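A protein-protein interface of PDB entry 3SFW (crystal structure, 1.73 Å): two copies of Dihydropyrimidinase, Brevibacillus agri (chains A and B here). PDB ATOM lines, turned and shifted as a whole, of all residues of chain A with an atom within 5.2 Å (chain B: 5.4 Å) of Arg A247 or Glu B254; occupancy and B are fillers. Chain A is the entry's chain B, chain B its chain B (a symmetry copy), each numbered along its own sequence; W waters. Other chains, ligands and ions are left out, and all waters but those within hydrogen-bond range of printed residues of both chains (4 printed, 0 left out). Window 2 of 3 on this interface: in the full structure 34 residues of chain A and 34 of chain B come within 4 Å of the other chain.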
ATOM      1  N   ALA A 243      35.032   2.782  15.041  1.00  0.00           N
ATOM      2  CA  ALA A 243      33.651   2.600  14.613  1.00  0.00           C
ATOM      3  C   ALA A 243      33.048   3.856  13.976  1.00  0.00           C
ATOM      4  O   ALA A 243      32.246   3.759  13.000  1.00  0.00           O
ATOM      5  CB  ALA A 243      32.844   2.152  15.787  1.00  0.00           C
ATOM      6  N   ASP A 244      33.454   5.038  14.453  1.00  0.00           N
ATOM      7  CA  ASP A 244      32.892   6.279  13.860  1.00  0.00           C
ATOM      8  C   ASP A 244      33.148   6.260  12.355  1.00  0.00           C
ATOM      9  O   ASP A 244      32.253   6.495  11.539  1.00  0.00           O
ATOM     10  CB  ASP A 244      33.491   7.550  14.473  1.00  0.00           C
ATOM     11  CG  ASP A 244      33.020   7.815  15.920  1.00  0.00           C
ATOM     12  OD1 ASP A 244      31.978   7.238  16.335  1.00  0.00           O
ATOM     13  OD2 ASP A 244      33.663   8.666  16.626  1.00  0.00           O
ATOM     14  N   ALA A 245      34.401   5.993  11.985  1.00  0.00           N
ATOM     15  CA  ALA A 245      34.756   5.947  10.566  1.00  0.00           C
ATOM     16  C   ALA A 245      34.097   4.797   9.799  1.00  0.00           C
ATOM     17  O   ALA A 245      33.678   4.984   8.644  1.00  0.00           O
ATOM     18  CB  ALA A 245      36.269   5.925  10.398  1.00  0.00           C
ATOM     19  N   VAL A 246      34.024   3.612  10.405  1.00  0.00           N
ATOM     20  CA  VAL A 246      33.405   2.438   9.742  1.00  0.00           C
ATOM     21  C   VAL A 246      31.952   2.789   9.406  1.00  0.00           C
ATOM     22  O   VAL A 246      31.430   2.422   8.363  1.00  0.00           O
ATOM     23  CB  VAL A 246      33.419   1.232  10.695  1.00  0.00           C
ATOM     24  CG1 VAL A 246      32.523   0.130  10.194  1.00  0.00           C
ATOM     25  CG2 VAL A 246      34.870   0.742  10.879  1.00  0.00           C
ATOM     26  N   ARG A 247      31.272   3.416  10.356  1.00  0.00           N
ATOM     27  CA  ARG A 247      29.846   3.723  10.149  1.00  0.00           C
ATOM     28  C   ARG A 247      29.674   4.607   8.914  1.00  0.00           C
ATOM     29  O   ARG A 247      28.765   4.405   8.111  1.00  0.00           O
ATOM     30  CB  ARG A 247      29.280   4.430  11.385  1.00  0.00           C
ATOM     31  CG  ARG A 247      29.139   3.475  12.615  1.00  0.00           C
ATOM     32  CD  ARG A 247      29.050   4.322  13.913  1.00  0.00           C
ATOM     33  NE  ARG A 247      29.196   3.467  15.093  1.00  0.00           N
ATOM     34  CZ  ARG A 247      29.354   3.948  16.325  1.00  0.00           C
ATOM     35  NH1 ARG A 247      29.338   5.267  16.512  1.00  0.00           N
ATOM     36  NH2 ARG A 247      29.445   3.123  17.362  1.00  0.00           N
ATOM     37  N   ARG A 248      30.544   5.606   8.764  1.00  0.00           N
ATOM     38  CA  ARG A 248      30.454   6.485   7.635  1.00  0.00           C
ATOM     39  C   ARG A 248      30.762   5.797   6.301  1.00  0.00           C
ATOM     40  O   ARG A 248      30.120   6.078   5.284  1.00  0.00           O
ATOM     41  CB  ARG A 248      31.393   7.655   7.839  1.00  0.00           C
ATOM     42  CG  ARG A 248      30.923   8.547   9.042  1.00  0.00           C
ATOM     43  CD  ARG A 248      31.950   9.559   9.291  1.00  0.00           C
ATOM     44  NE  ARG A 248      31.663  10.447  10.431  1.00  0.00           N
ATOM     45  CZ  ARG A 248      31.149  11.672  10.319  1.00  0.00           C
ATOM     46  NH1 ARG A 248      30.677  12.123   9.159  1.00  0.00           N
ATOM     47  NH2 ARG A 248      31.204  12.477  11.360  1.00  0.00           N
ATOM     48  N   ILE A 249      31.744   4.916   6.309  1.00  0.00           N
ATOM     49  CA  ILE A 249      32.062   4.132   5.104  1.00  0.00           C
ATOM     50  C   ILE A 249      30.891   3.198   4.765  1.00  0.00           C
ATOM     51  O   ILE A 249      30.527   3.055   3.573  1.00  0.00           O
ATOM     52  CB  ILE A 249      33.371   3.340   5.316  1.00  0.00           C
ATOM     53  CG1 ILE A 249      34.566   4.312   5.329  1.00  0.00           C
ATOM     54  CG2 ILE A 249      33.529   2.255   4.233  1.00  0.00           C
ATOM     55  CD1 ILE A 249      35.835   3.675   5.948  1.00  0.00           C
ATOM     56  N   ALA A 250      30.317   2.533   5.796  1.00  0.00           N
ATOM     57  CA  ALA A 250      29.167   1.625   5.560  1.00  0.00           C
ATOM     58  C   ALA A 250      28.016   2.407   4.903  1.00  0.00           C
ATOM     59  O   ALA A 250      27.389   1.955   3.927  1.00  0.00           O
ATOM     60  CB  ALA A 250      28.689   0.945   6.894  1.00  0.00           C
ATOM     61  N   GLU A 251      27.706   3.577   5.467  1.00  0.00           N
ATOM     62  CA  GLU A 251      26.652   4.441   4.914  1.00  0.00           C
ATOM     63  C   GLU A 251      26.945   4.837   3.446  1.00  0.00           C
ATOM     64  O   GLU A 251      26.035   4.775   2.577  1.00  0.00           O
ATOM     65  CB  GLU A 251      26.499   5.727   5.780  1.00  0.00           C
ATOM     66  CG  GLU A 251      25.481   6.735   5.214  1.00  0.00           C
ATOM     67  CD  GLU A 251      25.429   8.059   6.019  1.00  0.00           C
ATOM     68  OE1 GLU A 251      26.311   8.279   6.887  1.00  0.00           O
ATOM     69  OE2 GLU A 251      24.511   8.887   5.771  1.00  0.00           O
ATOM     70  N   ALA A 252      28.184   5.272   3.170  1.00  0.00           N
ATOM     71  CA  ALA A 252      28.544   5.650   1.780  1.00  0.00           C
ATOM     72  C   ALA A 252      28.346   4.480   0.824  1.00  0.00           C
ATOM     73  O   ALA A 252      27.875   4.662  -0.330  1.00  0.00           O
ATOM     74  CB  ALA A 252      30.019   6.128   1.700  1.00  0.00           C
ATOM     75  N   TRP A 295      36.790  -1.859  22.426  1.00  0.00           N
ATOM     76  CA  TRP A 295      35.535  -2.179  21.743  1.00  0.00           C
ATOM     77  C   TRP A 295      35.536  -1.875  20.231  1.00  0.00           C
ATOM     78  O   TRP A 295      34.757  -2.472  19.490  1.00  0.00           O
ATOM     79  CB  TRP A 295      34.306  -1.513  22.402  1.00  0.00           C
ATOM     80  CG  TRP A 295      34.243  -0.050  22.239  1.00  0.00           C
ATOM     81  CD1 TRP A 295      34.786   0.897  23.071  1.00  0.00           C
ATOM     82  CD2 TRP A 295      33.563   0.663  21.203  1.00  0.00           C
ATOM     83  NE1 TRP A 295      34.483   2.154  22.611  1.00  0.00           N
ATOM     84  CE2 TRP A 295      33.773   2.032  21.434  1.00  0.00           C
ATOM     85  CE3 TRP A 295      32.806   0.265  20.079  1.00  0.00           C
ATOM     86  CZ2 TRP A 295      33.194   3.033  20.632  1.00  0.00           C
ATOM     87  CZ3 TRP A 295      32.228   1.269  19.273  1.00  0.00           C
ATOM     88  CH2 TRP A 295      32.446   2.637  19.553  1.00  0.00           C
ATOM     89  N   VAL A 299      34.388  -4.012  15.930  1.00  0.00           N
ATOM     90  CA  VAL A 299      33.636  -3.325  14.862  1.00  0.00           C
ATOM     91  C   VAL A 299      34.439  -3.427  13.543  1.00  0.00           C
ATOM     92  O   VAL A 299      33.872  -3.654  12.468  1.00  0.00           O
ATOM     93  CB  VAL A 299      33.307  -1.845  15.203  1.00  0.00           C
ATOM     94  CG1 VAL A 299      32.522  -1.207  14.068  1.00  0.00           C
ATOM     95  CG2 VAL A 299      32.473  -1.764  16.486  1.00  0.00           C
ATOM     96  N   SER A 302      34.164  -7.002  12.313  1.00  0.00           N
ATOM     97  CA  SER A 302      32.819  -7.121  11.692  1.00  0.00           C
ATOM     98  C   SER A 302      32.818  -6.543  10.289  1.00  0.00           C
ATOM     99  O   SER A 302      32.144  -7.084   9.383  1.00  0.00           O
ATOM    100  CB  SER A 302      31.767  -6.381  12.504  1.00  0.00           C
ATOM    101  OG  SER A 302      31.486  -7.078  13.714  1.00  0.00           O
ATOM    102  N   ASN A 306      32.031  -8.584   6.938  1.00  0.00           N
ATOM    103  CA  ASN A 306      30.852  -8.257   6.117  1.00  0.00           C
ATOM    104  C   ASN A 306      31.118  -7.335   4.916  1.00  0.00           C
ATOM    105  O   ASN A 306      30.194  -6.856   4.261  1.00  0.00           O
ATOM    106  CB  ASN A 306      29.699  -7.760   7.030  1.00  0.00           C
ATOM    107  CG  ASN A 306      28.983  -8.897   7.734  1.00  0.00           C
ATOM    108  OD1 ASN A 306      29.065 -10.050   7.297  1.00  0.00           O
ATOM    109  ND2 ASN A 306      28.297  -8.595   8.856  1.00  0.00           N
ATOM    110  N   ILE A 308      32.592  -4.385   4.441  1.00  0.00           N
ATOM    111  CA  ILE A 308      32.560  -2.917   4.553  1.00  0.00           C
ATOM    112  C   ILE A 308      33.976  -2.304   4.494  1.00  0.00           C
ATOM    113  O   ILE A 308      34.164  -1.206   3.944  1.00  0.00           O
ATOM    114  CB  ILE A 308      31.873  -2.519   5.881  1.00  0.00           C
ATOM    115  CG1 ILE A 308      30.385  -2.919   5.830  1.00  0.00           C
ATOM    116  CG2 ILE A 308      32.038  -0.998   6.197  1.00  0.00           C
ATOM    117  CD1 ILE A 308      29.787  -3.028   7.225  1.00  0.00           C
ATOM    118  N   ILE B 249      19.217  -4.466   6.061  1.00  0.00           N
ATOM    119  CA  ILE B 249      20.274  -5.483   5.939  1.00  0.00           C
ATOM    120  C   ILE B 249      21.653  -4.822   6.076  1.00  0.00           C
ATOM    121  O   ILE B 249      22.552  -5.378   6.752  1.00  0.00           O
ATOM    122  CB  ILE B 249      20.139  -6.229   4.593  1.00  0.00           C
ATOM    123  CG1 ILE B 249      18.894  -7.136   4.628  1.00  0.00           C
ATOM    124  CG2 ILE B 249      21.420  -7.029   4.285  1.00  0.00           C
ATOM    125  CD1 ILE B 249      18.451  -7.580   3.212  1.00  0.00           C
ATOM    126  N   ALA B 250      21.844  -3.655   5.415  1.00  0.00           N
ATOM    127  CA  ALA B 250      23.141  -2.939   5.510  1.00  0.00           C
ATOM    128  C   ALA B 250      23.447  -2.615   6.983  1.00  0.00           C
ATOM    129  O   ALA B 250      24.572  -2.814   7.478  1.00  0.00           O
ATOM    130  CB  ALA B 250      23.139  -1.630   4.640  1.00  0.00           C
ATOM    131  N   GLU B 251      22.449  -2.071   7.682  1.00  0.00           N
ATOM    132  CA  GLU B 251      22.597  -1.749   9.110  1.00  0.00           C
ATOM    133  C   GLU B 251      22.957  -3.001   9.947  1.00  0.00           C
ATOM    134  O   GLU B 251      23.874  -2.947  10.810  1.00  0.00           O
ATOM    135  CB  GLU B 251      21.285  -1.115   9.660  1.00  0.00           C
ATOM    136  CG  GLU B 251      21.321  -0.837  11.174  1.00  0.00           C
ATOM    137  CD  GLU B 251      19.968  -0.320  11.727  1.00  0.00           C
ATOM    138  OE1 GLU B 251      18.951  -0.365  10.988  1.00  0.00           O
ATOM    139  OE2 GLU B 251      19.919   0.118  12.908  1.00  0.00           O
ATOM    140  N   ALA B 252      22.232  -4.108   9.727  1.00  0.00           N
ATOM    141  CA  ALA B 252      22.534  -5.353  10.478  1.00  0.00           C
ATOM    142  C   ALA B 252      23.970  -5.803  10.239  1.00  0.00           C
ATOM    143  O   ALA B 252      24.662  -6.277  11.178  1.00  0.00           O
ATOM    144  CB  ALA B 252      21.567  -6.496  10.068  1.00  0.00           C
ATOM    145  N   ARG B 253      24.412  -5.688   8.984  1.00  0.00           N
ATOM    146  CA  ARG B 253      25.732  -6.228   8.643  1.00  0.00           C
ATOM    147  C   ARG B 253      26.824  -5.329   9.218  1.00  0.00           C
ATOM    148  O   ARG B 253      27.907  -5.805   9.601  1.00  0.00           O
ATOM    149  CB  ARG B 253      25.853  -6.366   7.116  1.00  0.00           C
ATOM    150  CG  ARG B 253      25.103  -7.618   6.615  1.00  0.00           C
ATOM    151  CD  ARG B 253      25.112  -7.705   5.071  1.00  0.00           C
ATOM    152  NE  ARG B 253      26.468  -7.943   4.561  1.00  0.00           N
ATOM    153  CZ  ARG B 253      27.076  -9.139   4.507  1.00  0.00           C
ATOM    154  NH1 ARG B 253      26.460 -10.266   4.951  1.00  0.00           N
ATOM    155  NH2 ARG B 253      28.286  -9.210   3.963  1.00  0.00           N
ATOM    156  N   GLU B 254      26.539  -4.037   9.356  1.00  0.00           N
ATOM    157  CA  GLU B 254      27.557  -3.174   9.979  1.00  0.00           C
ATOM    158  C   GLU B 254      27.740  -3.486  11.473  1.00  0.00           C
ATOM    159  O   GLU B 254      28.826  -3.276  12.052  1.00  0.00           O
ATOM    160  CB  GLU B 254      27.247  -1.698   9.743  1.00  0.00           C
ATOM    161  CG  GLU B 254      28.398  -0.744  10.176  1.00  0.00           C
ATOM    162  CD  GLU B 254      28.313  -0.317  11.675  1.00  0.00           C
ATOM    163  OE1 GLU B 254      27.231  -0.469  12.283  1.00  0.00           O
ATOM    164  OE2 GLU B 254      29.368   0.099  12.269  1.00  0.00           O
ATOM    165  N   LYS B 255      26.685  -3.985  12.117  1.00  0.00           N
ATOM    166  CA  LYS B 255      26.812  -4.483  13.498  1.00  0.00           C
ATOM    167  C   LYS B 255      27.512  -5.809  13.621  1.00  0.00           C
ATOM    168  O   LYS B 255      27.713  -6.299  14.733  1.00  0.00           O
ATOM    169  CB  LYS B 255      25.428  -4.554  14.175  1.00  0.00           C
ATOM    170  CG  LYS B 255      24.743  -3.211  14.292  1.00  0.00           C
ATOM    171  CD  LYS B 255      23.386  -3.398  14.965  1.00  0.00           C
ATOM    172  CE  LYS B 255      22.517  -2.145  14.909  1.00  0.00           C
ATOM    173  NZ  LYS B 255      21.099  -2.556  15.196  1.00  0.00           N
ATOM    174  N   GLY B 256      27.800  -6.435  12.489  1.00  0.00           N
ATOM    175  CA  GLY B 256      28.506  -7.707  12.456  1.00  0.00           C
ATOM    176  C   GLY B 256      27.590  -8.924  12.519  1.00  0.00           C
ATOM    177  O   GLY B 256      28.075 -10.053  12.648  1.00  0.00           O
HETATM  178  O   HOH W   1      30.511  -4.947  15.274  1.00  0.00           O
HETATM  179  O   HOH W   2      29.233 -11.715   4.258  1.00  0.00           O
HETATM  180  O   HOH W   3      31.354  -3.139  10.960  1.00  0.00           O
HETATM  181  O   HOH W   4      27.382  -5.280   4.187  1.00  0.00           O
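Water W2 bridges the guanidinium group (NH2) of Arg B253 (2.7 Å) and the side-chain amide oxygen (OD1) of Asn A306 (3.5 Å).
Water W3 bridges the backbone carbonyl oxygen (O) of Glu B254 (2.8 Å) and the backbone carbonyl oxygen (O) of Val A299 (3.0 Å).
Water W1 bridges OG of Ser A302 (2.8 Å) and O of Lys B255 (3.2 Å).
Water W4 lies within hydrogen-bond range of NE of Arg B253 (2.8 Å) and O of Asn A306 (3.2 Å).
NH1 of Arg A247 lies within salt-bridge range of OD1 of Asp A244 (3.3 Å).
The side-chain carboxylate (OE2) of Glu B251 is in salt-bridge range of the side-chain amino group (NZ) of Lys B255, 3.7 Å away.
OE2 of Glu B254 touches CG1 of Val A246, at 3.8 Å.
Arg A247 touches Glu B254 (CG to OE2, 3.4 Å).
Ala A250 touches Glu B254.
Glu B254 touches Val A299 (OE2 to CG1, 3.9 Å).
Lys B255 touches Ser A302.
OG of Ser A302 touches CA of Gly B256, at 3.3 Å.
Gly B256 touches Asn A306.
Glu B254 touches Ile A308 (CA to CD1, 3.5 Å).
Arg A247 touches just one residue of chain B: Glu B254 (3.4 Å).
Of the printed residues of chain B, Ala A250 touches Glu B254 (3.7 Å).
Of the printed residues of chain B, Val A299 touches Glu B254.
Ala B252 touches none of the printed residues of chain A.
Glu B254 touches five residues of chain A.
The nearest residue of chain A that does not touch Glu B254 is Ser A302 (4.3 Å).
The nearest printed residue of chain B that does not touch Ile A308 is Arg B253 (4.1 Å).
Of the 8 printed residues of chain B, 4 touch a printed residue of chain A.
Among the printed residues, 9 pairs touch across the chains.
Among the printed residues, no Asp or Glu carboxylate lies within 4 Å of a Lys or Arg side-chain nitrogen of the other chain.
The side-chain amide nitrogen (ND2) of Asn A306 is in hydrogen-bond range of the backbone carbonyl oxygen (O) of Arg B253 (2.9 Å).
Positions printed for both chains: 249, 250, 251 and 252.
Of the 9 pairs that touch across the chains among the printed residues, none has its exchanged pair printed and touching as well.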
